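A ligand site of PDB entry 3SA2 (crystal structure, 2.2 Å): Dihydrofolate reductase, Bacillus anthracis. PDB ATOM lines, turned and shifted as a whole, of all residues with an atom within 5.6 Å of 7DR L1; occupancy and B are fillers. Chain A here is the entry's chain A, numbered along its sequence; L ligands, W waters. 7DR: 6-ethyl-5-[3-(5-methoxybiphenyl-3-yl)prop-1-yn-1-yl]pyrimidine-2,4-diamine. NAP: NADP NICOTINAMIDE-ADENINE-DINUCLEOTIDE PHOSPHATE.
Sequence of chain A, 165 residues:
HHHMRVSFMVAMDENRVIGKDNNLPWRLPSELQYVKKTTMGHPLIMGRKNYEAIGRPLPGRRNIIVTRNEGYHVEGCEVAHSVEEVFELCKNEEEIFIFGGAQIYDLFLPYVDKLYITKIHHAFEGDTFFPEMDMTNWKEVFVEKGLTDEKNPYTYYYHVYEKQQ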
ATOM      1  N   MET A   9      31.507 -21.181 -12.295  1.00  0.00           N
ATOM      2  CA  MET A   9      31.495 -20.224 -11.206  1.00  0.00           C
ATOM      3  C   MET A   9      30.247 -20.506 -10.390  1.00  0.00           C
ATOM      4  O   MET A   9      29.130 -20.413 -10.907  1.00  0.00           O
ATOM      5  CB  MET A   9      31.509 -18.793 -11.740  1.00  0.00           C
ATOM      6  CG  MET A   9      31.257 -17.697 -10.691  1.00  0.00           C
ATOM      7  SD  MET A   9      32.521 -17.556  -9.378  1.00  0.00           S
ATOM      8  CE  MET A   9      33.985 -17.110 -10.344  1.00  0.00           C
ATOM      9  N   VAL A  10      30.444 -20.868  -9.114  1.00  0.00           N
ATOM     10  CA  VAL A  10      29.344 -21.307  -8.254  1.00  0.00           C
ATOM     11  C   VAL A  10      29.639 -21.062  -6.777  1.00  0.00           C
ATOM     12  O   VAL A  10      30.787 -21.158  -6.333  1.00  0.00           O
ATOM     13  CB  VAL A  10      28.975 -22.805  -8.496  1.00  0.00           C
ATOM     14  CG1 VAL A  10      30.095 -23.751  -8.053  1.00  0.00           C
ATOM     15  CG2 VAL A  10      27.655 -23.176  -7.819  1.00  0.00           C
ATOM     16  N   ALA A  11      28.597 -20.727  -6.020  1.00  0.00           N
ATOM     17  CA  ALA A  11      28.656 -20.703  -4.553  1.00  0.00           C
ATOM     18  C   ALA A  11      27.665 -21.731  -4.021  1.00  0.00           C
ATOM     19  O   ALA A  11      26.508 -21.730  -4.435  1.00  0.00           O
ATOM     20  CB  ALA A  11      28.305 -19.309  -4.050  1.00  0.00           C
ATOM     21  N   ASN A  22      13.735 -20.365  -6.474  1.00  0.00           N
ATOM     22  CA  ASN A  22      14.229 -19.640  -7.659  1.00  0.00           C
ATOM     23  C   ASN A  22      15.049 -18.389  -7.335  1.00  0.00           C
ATOM     24  O   ASN A  22      15.137 -17.452  -8.132  1.00  0.00           O
ATOM     25  CB  ASN A  22      13.069 -19.330  -8.631  1.00  0.00           C
ATOM     26  CG  ASN A  22      13.528 -19.142 -10.070  1.00  0.00           C
ATOM     27  OD1 ASN A  22      14.404 -19.861 -10.570  1.00  0.00           O
ATOM     28  ND2 ASN A  22      12.932 -18.182 -10.760  1.00  0.00           N
ATOM     29  N   ASN A  23      15.656 -18.388  -6.140  1.00  0.00           N
ATOM     30  CA  ASN A  23      16.539 -17.312  -5.719  1.00  0.00           C
ATOM     31  C   ASN A  23      17.733 -17.877  -4.923  1.00  0.00           C
ATOM     32  O   ASN A  23      17.842 -19.093  -4.750  1.00  0.00           O
ATOM     33  CB  ASN A  23      15.757 -16.288  -4.885  1.00  0.00           C
ATOM     34  CG  ASN A  23      16.297 -14.856  -5.048  1.00  0.00           C
ATOM     35  OD1 ASN A  23      17.479 -14.637  -5.357  1.00  0.00           O
ATOM     36  ND2 ASN A  23      15.418 -13.875  -4.824  1.00  0.00           N
ATOM     37  N   LEU A  24      18.612 -16.994  -4.459  1.00  0.00           N
ATOM     38  CA  LEU A  24      19.745 -17.362  -3.620  1.00  0.00           C
ATOM     39  C   LEU A  24      19.322 -17.456  -2.153  1.00  0.00           C
ATOM     40  O   LEU A  24      18.613 -16.582  -1.686  1.00  0.00           O
ATOM     41  CB  LEU A  24      20.867 -16.331  -3.768  1.00  0.00           C
ATOM     42  CG  LEU A  24      21.473 -16.193  -5.165  1.00  0.00           C
ATOM     43  CD1 LEU A  24      22.433 -15.020  -5.202  1.00  0.00           C
ATOM     44  CD2 LEU A  24      22.182 -17.499  -5.575  1.00  0.00           C
ATOM     45  N   TRP A  26      21.140 -17.091   0.510  1.00  0.00           N
ATOM     46  CA  TRP A  26      21.939 -16.227   1.384  1.00  0.00           C
ATOM     47  C   TRP A  26      22.238 -14.907   0.690  1.00  0.00           C
ATOM     48  O   TRP A  26      22.027 -14.764  -0.524  1.00  0.00           O
ATOM     49  CB  TRP A  26      23.278 -16.906   1.709  1.00  0.00           C
ATOM     50  CG  TRP A  26      24.007 -17.347   0.453  1.00  0.00           C
ATOM     51  CD1 TRP A  26      24.762 -16.558  -0.365  1.00  0.00           C
ATOM     52  CD2 TRP A  26      24.005 -18.647  -0.142  1.00  0.00           C
ATOM     53  NE1 TRP A  26      25.249 -17.297  -1.422  1.00  0.00           N
ATOM     54  CE2 TRP A  26      24.787 -18.585  -1.308  1.00  0.00           C
ATOM     55  CE3 TRP A  26      23.420 -19.884   0.206  1.00  0.00           C
ATOM     56  CZ2 TRP A  26      25.009 -19.706  -2.139  1.00  0.00           C
ATOM     57  CZ3 TRP A  26      23.636 -20.984  -0.619  1.00  0.00           C
ATOM     58  CH2 TRP A  26      24.429 -20.884  -1.774  1.00  0.00           C
ATOM     59  N   GLU A  31      31.189 -11.844  -1.377  1.00  0.00           N
ATOM     60  CA  GLU A  31      31.295 -12.974  -2.281  1.00  0.00           C
ATOM     61  C   GLU A  31      30.895 -12.576  -3.702  1.00  0.00           C
ATOM     62  O   GLU A  31      31.499 -13.023  -4.668  1.00  0.00           O
ATOM     63  CB  GLU A  31      30.409 -14.118  -1.779  1.00  0.00           C
ATOM     64  CG  GLU A  31      30.872 -15.510  -2.188  1.00  0.00           C
ATOM     65  CD  GLU A  31      30.463 -15.899  -3.603  1.00  0.00           C
ATOM     66  OE1 GLU A  31      29.359 -15.499  -4.047  1.00  0.00           O
ATOM     67  OE2 GLU A  31      31.244 -16.617  -4.266  1.00  0.00           O
ATOM     68  N   LEU A  32      29.867 -11.737  -3.805  1.00  0.00           N
ATOM     69  CA  LEU A  32      29.448 -11.154  -5.092  1.00  0.00           C
ATOM     70  C   LEU A  32      30.562 -10.326  -5.738  1.00  0.00           C
ATOM     71  O   LEU A  32      30.741 -10.386  -6.957  1.00  0.00           O
ATOM     72  CB  LEU A  32      28.219 -10.279  -4.893  1.00  0.00           C
ATOM     73  CG  LEU A  32      27.504  -9.718  -6.117  1.00  0.00           C
ATOM     74  CD1 LEU A  32      26.794 -10.829  -6.853  1.00  0.00           C
ATOM     75  CD2 LEU A  32      26.508  -8.599  -5.712  1.00  0.00           C
ATOM     76  N   TYR A  34      33.821 -10.706  -5.300  1.00  0.00           N
ATOM     77  CA  TYR A  34      34.765 -11.699  -5.808  1.00  0.00           C
ATOM     78  C   TYR A  34      34.290 -12.260  -7.158  1.00  0.00           C
ATOM     79  O   TYR A  34      35.094 -12.414  -8.071  1.00  0.00           O
ATOM     80  CB  TYR A  34      34.934 -12.820  -4.800  1.00  0.00           C
ATOM     81  CG  TYR A  34      35.678 -14.034  -5.300  1.00  0.00           C
ATOM     82  CD1 TYR A  34      37.072 -14.120  -5.166  1.00  0.00           C
ATOM     83  CD2 TYR A  34      35.008 -15.099  -5.901  1.00  0.00           C
ATOM     84  CE1 TYR A  34      37.768 -15.242  -5.631  1.00  0.00           C
ATOM     85  CE2 TYR A  34      35.695 -16.223  -6.368  1.00  0.00           C
ATOM     86  CZ  TYR A  34      37.070 -16.284  -6.223  1.00  0.00           C
ATOM     87  OH  TYR A  34      37.747 -17.395  -6.663  1.00  0.00           O
ATOM     88  N   VAL A  35      32.997 -12.549  -7.259  1.00  0.00           N
ATOM     89  CA  VAL A  35      32.388 -12.984  -8.514  1.00  0.00           C
ATOM     90  C   VAL A  35      32.586 -11.964  -9.638  1.00  0.00           C
ATOM     91  O   VAL A  35      32.969 -12.342 -10.745  1.00  0.00           O
ATOM     92  CB  VAL A  35      30.891 -13.317  -8.325  1.00  0.00           C
ATOM     93  CG1 VAL A  35      30.187 -13.477  -9.674  1.00  0.00           C
ATOM     94  CG2 VAL A  35      30.749 -14.568  -7.480  1.00  0.00           C
ATOM     95  N   LYS A  36      32.337 -10.683  -9.362  1.00  0.00           N
ATOM     96  CA  LYS A  36      32.490  -9.606 -10.356  1.00  0.00           C
ATOM     97  C   LYS A  36      33.944  -9.486 -10.783  1.00  0.00           C
ATOM     98  O   LYS A  36      34.260  -9.482 -11.973  1.00  0.00           O
ATOM     99  CB  LYS A  36      31.947  -8.272  -9.838  1.00  0.00           C
ATOM    100  CG  LYS A  36      30.454  -8.293  -9.498  1.00  0.00           C
ATOM    101  CD  LYS A  36      29.897  -6.900  -9.178  1.00  0.00           C
ATOM    102  CE  LYS A  36      28.444  -6.998  -8.728  1.00  0.00           C
ATOM    103  NZ  LYS A  36      27.785  -5.649  -8.589  1.00  0.00           N
ATOM    104  N   ASN A  50      17.994 -18.823 -14.250  1.00  0.00           N
ATOM    105  CA  ASN A  50      19.024 -18.010 -13.620  1.00  0.00           C
ATOM    106  C   ASN A  50      18.997 -16.580 -14.158  1.00  0.00           C
ATOM    107  O   ASN A  50      18.898 -15.630 -13.382  1.00  0.00           O
ATOM    108  CB  ASN A  50      20.428 -18.618 -13.808  1.00  0.00           C
ATOM    109  CG  ASN A  50      21.521 -17.841 -13.069  1.00  0.00           C
ATOM    110  OD1 ASN A  50      21.242 -17.098 -12.127  1.00  0.00           O
ATOM    111  ND2 ASN A  50      22.765 -18.009 -13.515  1.00  0.00           N
ATOM    112  N   ALA A  53      15.923 -14.318 -13.087  1.00  0.00           N
ATOM    113  CA  ALA A  53      16.019 -13.920 -11.692  1.00  0.00           C
ATOM    114  C   ALA A  53      16.994 -12.748 -11.543  1.00  0.00           C
ATOM    115  O   ALA A  53      16.744 -11.800 -10.791  1.00  0.00           O
ATOM    116  CB  ALA A  53      16.419 -15.089 -10.810  1.00  0.00           C
ATOM    117  N   ILE A  54      18.120 -12.814 -12.263  1.00  0.00           N
ATOM    118  CA  ILE A  54      19.059 -11.696 -12.300  1.00  0.00           C
ATOM    119  C   ILE A  54      18.331 -10.457 -12.824  1.00  0.00           C
ATOM    120  O   ILE A  54      18.316  -9.412 -12.162  1.00  0.00           O
ATOM    121  CB  ILE A  54      20.322 -12.031 -13.134  1.00  0.00           C
ATOM    122  CG1 ILE A  54      21.090 -13.188 -12.466  1.00  0.00           C
ATOM    123  CG2 ILE A  54      21.210 -10.788 -13.275  1.00  0.00           C
ATOM    124  CD1 ILE A  54      22.194 -13.779 -13.299  1.00  0.00           C
ATOM    125  N   ARG A  56      18.561  -8.516 -15.657  1.00  0.00           N
ATOM    126  CA  ARG A  56      19.212  -7.488 -16.463  1.00  0.00           C
ATOM    127  C   ARG A  56      20.558  -8.005 -16.991  1.00  0.00           C
ATOM    128  O   ARG A  56      21.178  -8.853 -16.356  1.00  0.00           O
ATOM    129  CB  ARG A  56      19.418  -6.195 -15.634  1.00  0.00           C
ATOM    130  CG  ARG A  56      20.502  -6.324 -14.551  1.00  0.00           C
ATOM    131  CD  ARG A  56      20.436  -5.241 -13.477  1.00  0.00           C
ATOM    132  NE  ARG A  56      21.639  -5.233 -12.636  1.00  0.00           N
ATOM    133  CZ  ARG A  56      21.885  -6.065 -11.627  1.00  0.00           C
ATOM    134  NH1 ARG A  56      21.011  -7.014 -11.283  1.00  0.00           N
ATOM    135  NH2 ARG A  56      23.011  -5.952 -10.940  1.00  0.00           N
ATOM    136  N   LEU A  58      24.411  -8.131 -17.300  1.00  0.00           N
ATOM    137  CA  LEU A  58      25.527  -7.716 -16.443  1.00  0.00           C
ATOM    138  C   LEU A  58      26.590  -7.009 -17.289  1.00  0.00           C
ATOM    139  O   LEU A  58      27.034  -7.540 -18.306  1.00  0.00           O
ATOM    140  CB  LEU A  58      26.103  -8.917 -15.687  1.00  0.00           C
ATOM    141  CG  LEU A  58      25.113  -9.680 -14.796  1.00  0.00           C
ATOM    142  CD1 LEU A  58      25.828 -10.782 -14.044  1.00  0.00           C
ATOM    143  CD2 LEU A  58      24.380  -8.761 -13.822  1.00  0.00           C
ATOM    144  N   ILE A  98      30.562 -20.732 -16.782  1.00  0.00           N
ATOM    145  CA  ILE A  98      29.255 -21.323 -16.592  1.00  0.00           C
ATOM    146  C   ILE A  98      28.766 -20.826 -15.252  1.00  0.00           C
ATOM    147  O   ILE A  98      29.351 -21.149 -14.205  1.00  0.00           O
ATOM    148  CB  ILE A  98      29.296 -22.874 -16.667  1.00  0.00           C
ATOM    149  CG1 ILE A  98      30.099 -23.350 -17.898  1.00  0.00           C
ATOM    150  CG2 ILE A  98      27.885 -23.452 -16.699  1.00  0.00           C
ATOM    151  CD1 ILE A  98      29.588 -22.872 -19.271  1.00  0.00           C
ATOM    152  N   PHE A  99      27.700 -20.030 -15.300  1.00  0.00           N
ATOM    153  CA  PHE A  99      27.227 -19.223 -14.185  1.00  0.00           C
ATOM    154  C   PHE A  99      25.980 -19.780 -13.482  1.00  0.00           C
ATOM    155  O   PHE A  99      25.443 -19.133 -12.564  1.00  0.00           O
ATOM    156  CB  PHE A  99      26.940 -17.816 -14.716  1.00  0.00           C
ATOM    157  CG  PHE A  99      26.977 -16.720 -13.682  1.00  0.00           C
ATOM    158  CD1 PHE A  99      28.146 -16.483 -12.936  1.00  0.00           C
ATOM    159  CD2 PHE A  99      25.877 -15.878 -13.511  1.00  0.00           C
ATOM    160  CE1 PHE A  99      28.202 -15.457 -12.002  1.00  0.00           C
ATOM    161  CE2 PHE A  99      25.916 -14.833 -12.573  1.00  0.00           C
ATOM    162  CZ  PHE A  99      27.079 -14.626 -11.815  1.00  0.00           C
ATOM    163  N   GLY A 100      25.519 -20.960 -13.903  1.00  0.00           N
ATOM    164  CA  GLY A 100      24.345 -21.599 -13.294  1.00  0.00           C
ATOM    165  C   GLY A 100      23.045 -21.393 -14.050  1.00  0.00           C
ATOM    166  O   GLY A 100      23.032 -20.710 -15.071  1.00  0.00           O
ATOM    167  N   TYR A 105      24.571 -26.257 -15.020  1.00  0.00           N
ATOM    168  CA  TYR A 105      25.787 -26.923 -14.514  1.00  0.00           C
ATOM    169  C   TYR A 105      25.828 -28.377 -14.951  1.00  0.00           C
ATOM    170  O   TYR A 105      26.893 -28.883 -15.293  1.00  0.00           O
ATOM    171  CB  TYR A 105      25.896 -26.866 -12.982  1.00  0.00           C
ATOM    172  CG  TYR A 105      26.142 -25.489 -12.410  1.00  0.00           C
ATOM    173  CD1 TYR A 105      27.130 -24.663 -12.935  1.00  0.00           C
ATOM    174  CD2 TYR A 105      25.412 -25.043 -11.322  1.00  0.00           C
ATOM    175  CE1 TYR A 105      27.366 -23.411 -12.392  1.00  0.00           C
ATOM    176  CE2 TYR A 105      25.645 -23.792 -10.766  1.00  0.00           C
ATOM    177  CZ  TYR A 105      26.621 -22.984 -11.309  1.00  0.00           C
ATOM    178  OH  TYR A 105      26.841 -21.735 -10.785  1.00  0.00           O
ATOM    179  N   TYR A 116      35.686 -22.686 -10.042  1.00  0.00           N
ATOM    180  CA  TYR A 116      35.723 -21.669  -8.989  1.00  0.00           C
ATOM    181  C   TYR A 116      34.505 -21.872  -8.105  1.00  0.00           C
ATOM    182  O   TYR A 116      33.373 -21.498  -8.462  1.00  0.00           O
ATOM    183  CB  TYR A 116      35.687 -20.249  -9.566  1.00  0.00           C
ATOM    184  CG  TYR A 116      36.759 -19.911 -10.562  1.00  0.00           C
ATOM    185  CD1 TYR A 116      36.749 -20.464 -11.839  1.00  0.00           C
ATOM    186  CD2 TYR A 116      37.769 -18.997 -10.261  1.00  0.00           C
ATOM    187  CE1 TYR A 116      37.715 -20.146 -12.774  1.00  0.00           C
ATOM    188  CE2 TYR A 116      38.751 -18.669 -11.185  1.00  0.00           C
ATOM    189  CZ  TYR A 116      38.711 -19.249 -12.448  1.00  0.00           C
ATOM    190  OH  TYR A 116      39.674 -18.925 -13.377  1.00  0.00           O
ATOM    191  N   THR A 118      32.845 -21.439  -4.296  1.00  0.00           N
ATOM    192  CA  THR A 118      32.790 -20.913  -2.949  1.00  0.00           C
ATOM    193  C   THR A 118      32.019 -21.899  -2.077  1.00  0.00           C
ATOM    194  O   THR A 118      30.925 -22.332  -2.432  1.00  0.00           O
ATOM    195  CB  THR A 118      32.116 -19.518  -2.906  1.00  0.00           C
ATOM    196  OG1 THR A 118      32.865 -18.622  -3.743  1.00  0.00           O
ATOM    197  CG2 THR A 118      32.083 -18.972  -1.494  1.00  0.00           C
HETATM  198  N1  7DR L   1      28.978 -18.063  -8.256  1.00  0.00           N
HETATM  199  C2  7DR L   1      29.321 -17.624  -7.038  1.00  0.00           C
HETATM  200  N3  7DR L   1      28.461 -16.907  -6.308  1.00  0.00           N
HETATM  201  C4  7DR L   1      27.225 -16.591  -6.744  1.00  0.00           C
HETATM  202  C5  7DR L   1      26.853 -17.043  -8.006  1.00  0.00           C
HETATM  203  C6  7DR L   1      27.757 -17.788  -8.763  1.00  0.00           C
HETATM  204  CAA 7DR L   1      26.497 -14.282  -6.076  1.00  0.00           C
HETATM  205  CAB 7DR L   1      18.886 -13.664  -8.112  1.00  0.00           C
HETATM  206  NAC 7DR L   1      30.519 -17.904  -6.522  1.00  0.00           N
HETATM  207  NAD 7DR L   1      27.426 -18.232  -9.985  1.00  0.00           N
HETATM  208  CAE 7DR L   1      24.403 -16.428  -8.911  1.00  0.00           C
HETATM  209  CAF 7DR L   1      25.536 -16.722  -8.500  1.00  0.00           C
HETATM  210  CAG 7DR L   1      25.946  -9.164 -10.352  1.00  0.00           C
HETATM  211  CAH 7DR L   1      26.312 -10.493 -10.557  1.00  0.00           C
HETATM  212  CAI 7DR L   1      24.671  -8.866  -9.887  1.00  0.00           C
HETATM  213  CAJ 7DR L   1      25.409 -11.514 -10.288  1.00  0.00           C
HETATM  214  CAK 7DR L   1      23.767  -9.894  -9.611  1.00  0.00           C
HETATM  215  CAL 7DR L   1      21.378 -14.258  -8.940  1.00  0.00           C
HETATM  216  CAM 7DR L   1      23.592 -13.600  -9.594  1.00  0.00           C
HETATM  217  CAN 7DR L   1      21.915 -11.918  -9.157  1.00  0.00           C
HETATM  218  CAO 7DR L   1      26.322 -15.771  -5.810  1.00  0.00           C
HETATM  219  CAP 7DR L   1      23.048 -16.093  -9.391  1.00  0.00           C
HETATM  220  OAS 7DR L   1      19.718 -12.544  -8.512  1.00  0.00           O
HETATM  221  CAU 7DR L   1      22.679 -14.608  -9.298  1.00  0.00           C
HETATM  222  CAW 7DR L   1      20.990 -12.914  -8.864  1.00  0.00           C
HETATM  223  CAX 7DR L   1      24.133 -11.230  -9.810  1.00  0.00           C
HETATM  224  CAY 7DR L   1      23.216 -12.253  -9.529  1.00  0.00           C
HETATM  225  PA  NAP L   2      18.701 -22.857 -14.702  1.00  0.00           P
HETATM  226  O1A NAP L   2      19.613 -24.003 -14.881  1.00  0.00           O
HETATM  227  O2A NAP L   2      19.377 -21.578 -14.457  1.00  0.00           O
HETATM  228  O5B NAP L   2      17.765 -22.679 -15.988  1.00  0.00           O
HETATM  229  C5B NAP L   2      16.968 -23.761 -16.409  1.00  0.00           C
HETATM  230  C4B NAP L   2      16.565 -23.486 -17.842  1.00  0.00           C
HETATM  231  O4B NAP L   2      17.697 -23.638 -18.680  1.00  0.00           O
HETATM  232  C3B NAP L   2      15.516 -24.418 -18.423  1.00  0.00           C
HETATM  233  O3B NAP L   2      14.202 -24.078 -18.047  1.00  0.00           O
HETATM  234  C2B NAP L   2      15.743 -24.176 -19.904  1.00  0.00           C
HETATM  235  O2B NAP L   2      15.177 -22.947 -20.314  1.00  0.00           O
HETATM  236  C1B NAP L   2      17.269 -24.066 -19.948  1.00  0.00           C
HETATM  237  N9A NAP L   2      17.813 -25.411 -20.262  1.00  0.00           N
HETATM  238  C8A NAP L   2      17.980 -26.469 -19.420  1.00  0.00           C
HETATM  239  N7A NAP L   2      18.481 -27.504 -20.135  1.00  0.00           N
HETATM  240  C5A NAP L   2      18.629 -27.124 -21.419  1.00  0.00           C
HETATM  241  C6A NAP L   2      19.098 -27.774 -22.558  1.00  0.00           C
HETATM  242  N6A NAP L   2      19.514 -29.038 -22.522  1.00  0.00           N
HETATM  243  N1A NAP L   2      19.139 -27.082 -23.755  1.00  0.00           N
HETATM  244  C2A NAP L   2      18.724 -25.774 -23.833  1.00  0.00           C
HETATM  245  N3A NAP L   2      18.261 -25.145 -22.700  1.00  0.00           N
HETATM  246  C4A NAP L   2      18.215 -25.802 -21.511  1.00  0.00           C
HETATM  247  O3  NAP L   2      17.619 -23.246 -13.587  1.00  0.00           O
HETATM  248  PN  NAP L   2      17.689 -24.043 -12.205  1.00  0.00           P
HETATM  249  O1N NAP L   2      16.329 -24.091 -11.629  1.00  0.00           O
HETATM  250  O2N NAP L   2      18.449 -25.292 -12.411  1.00  0.00           O
HETATM  251  O5D NAP L   2      18.630 -23.056 -11.328  1.00  0.00           O
HETATM  252  C5D NAP L   2      18.097 -21.850 -10.827  1.00  0.00           C
HETATM  253  C4D NAP L   2      18.340 -21.789  -9.327  1.00  0.00           C
HETATM  254  O4D NAP L   2      19.733 -21.888  -9.018  1.00  0.00           O
HETATM  255  C3D NAP L   2      17.867 -20.448  -8.798  1.00  0.00           C
HETATM  256  O3D NAP L   2      17.444 -20.674  -7.468  1.00  0.00           O
HETATM  257  C2D NAP L   2      19.142 -19.637  -8.792  1.00  0.00           C
HETATM  258  O2D NAP L   2      19.107 -18.557  -7.879  1.00  0.00           O
HETATM  259  C1D NAP L   2      20.156 -20.684  -8.387  1.00  0.00           C
HETATM  260  N1N NAP L   2      21.526 -20.342  -8.746  1.00  0.00           N
HETATM  261  C2N NAP L   2      22.458 -20.300  -7.738  1.00  0.00           C
HETATM  262  C3N NAP L   2      23.787 -20.016  -8.015  1.00  0.00           C
HETATM  263  C7N NAP L   2      24.828 -20.095  -6.926  1.00  0.00           C
HETATM  264  O7N NAP L   2      26.179 -19.981  -7.276  1.00  0.00           O
HETATM  265  N7N NAP L   2      24.461 -20.260  -5.659  1.00  0.00           N
HETATM  266  C4N NAP L   2      24.160 -19.764  -9.334  1.00  0.00           C
HETATM  267  C5N NAP L   2      23.210 -19.803 -10.354  1.00  0.00           C
HETATM  268  C6N NAP L   2      21.880 -20.108 -10.057  1.00  0.00           C
HETATM  269  P2B NAP L   2      13.703 -22.818 -20.985  1.00  0.00           P
HETATM  270  O1X NAP L   2      12.702 -23.322 -19.970  1.00  0.00           O
HETATM  271  O2X NAP L   2      13.419 -21.379 -21.310  1.00  0.00           O
HETATM  272  O3X NAP L   2      13.585 -23.674 -22.220  1.00  0.00           O
HETATM  273  O   HOH W   1      26.964 -15.772  -2.586  1.00  0.00           O
HETATM  274  O   HOH W   2      33.547 -19.047  -6.338  1.00  0.00           O
HETATM  275  O   HOH W   3      19.419 -16.750 -10.025  1.00  0.00           O
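OE2 of Glu 31 lies within hydrogen-bond range of NAC of 7DR L1.
An oxygen (O7N) of NAP L2 sits at hydrogen-bond distance from the backbone NH of Ala 11, at 2.8 Å.
N of Val 10 sits close to N1 of 7DR L1, at 3.3 Å.
A nitrogen (N7N) of NAP L2 lies within hydrogen-bond range of the backbone carbonyl oxygen of Ala 11 (2.8 Å).
The backbone carbonyl oxygen (O) of Asn 23 lies within hydrogen-bond range of an oxygen (O3D) of NAP L2 (3.2 Å).
O2A of NAP L2 sits at hydrogen-bond distance from N of Asn 50.
A nitrogen (NAC) of 7DR L1 is in hydrogen-bond range of the backbone carbonyl oxygen (O) of Val 10, at 3.3 Å.
NAD of 7DR L1 sits at hydrogen-bond distance from O of Phe 99 (3.4 Å).
The backbone NH (N) of Ala 11 sits close to a nitrogen (N1) of 7DR L1 (3.5 Å).
A nitrogen (NAD) of 7DR L1 is in hydrogen-bond range of the backbone carbonyl oxygen (O) of Met 9 (2.9 Å).
A nitrogen (NAC) of 7DR L1 is in hydrogen-bond range of the side-chain sulfur of Met 9, 3.5 Å away.
N of Asn 23 lies within hydrogen-bond range of O3D of NAP L2.
A nitrogen (NAD) of 7DR L1 lies close to an oxygen (O7N) of NAP L2 (3.5 Å).
The side-chain hydroxyl of Tyr 105 lies close to the backbone NH of Gly 100, 3.5 Å away.
OH of Tyr 105 sits at hydrogen-bond distance from O of Met 9.
N of Val 10 is in hydrogen-bond range of O of Tyr 116 (3.1 Å).
The side-chain hydroxyl of Tyr 105 sits close to the backbone carbonyl oxygen of Phe 99, 3.4 Å away.
The backbone carbonyl oxygen (O) of Val 10 sits at hydrogen-bond distance from the backbone NH (N) of Thr 118, 2.9 Å away.
The side-chain hydroxyl (OG1) of Thr 118 lies within hydrogen-bond range of the side-chain carboxylate (OE2) of Glu 31 (2.6 Å).
N of Met 9 is in hydrogen-bond range of O of Ile 98, 2.9 Å away.
The backbone carbonyl oxygen of Gly 100 sits at hydrogen-bond distance from the side-chain amide nitrogen of Asn 50 (3.1 Å).
Asn 23 touches 7DR L1.
Leu 24 touches 7DR L1 (CD1 to CAL, 3.96 Å).
Leu 32 touches 7DR L1.
CG2 of Val 35 touches C2 of 7DR L1, 3.4 Å away.
CE of Lys 36 touches CAG of 7DR L1, 3.7 Å away.
OD1 of Asn 50 touches CAP of 7DR L1, 3.4 Å away.
Ala 53 touches 7DR L1 (O to OAS, 3.8 Å).
Ile 54 touches 7DR L1.
NH2 of Arg 56 touches CAI of 7DR L1, 3.5 Å away.
Leu 58 touches 7DR L1.
OH of Tyr 105 touches NAD of 7DR L1, at 3.6 Å.
OG1 of Thr 118 touches NAC of 7DR L1, 3.7 Å away.
17 residues have an atom within 4 Å of 7DR L1: Met 9, Val 10, Ala 11, Asn 23, Leu 24, Glu 31, Leu 32, Val 35, Lys 36, Asn 50, Ala 53, Ile 54, Arg 56, Leu 58, Phe 99, Tyr 105 and Thr 118.
The nearest printed residue that does not touch 7DR L1 is Trp 26 (4.8 Å).
Water W1 lies within hydrogen-bond range of NE1 of Trp 26 and OE1 of Glu 31.
Water W3 lies within hydrogen-bond range of the side-chain amide oxygen of Asn 50 (2.8 Å) and an oxygen (O2D) of NAP L2 (2.8 Å).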
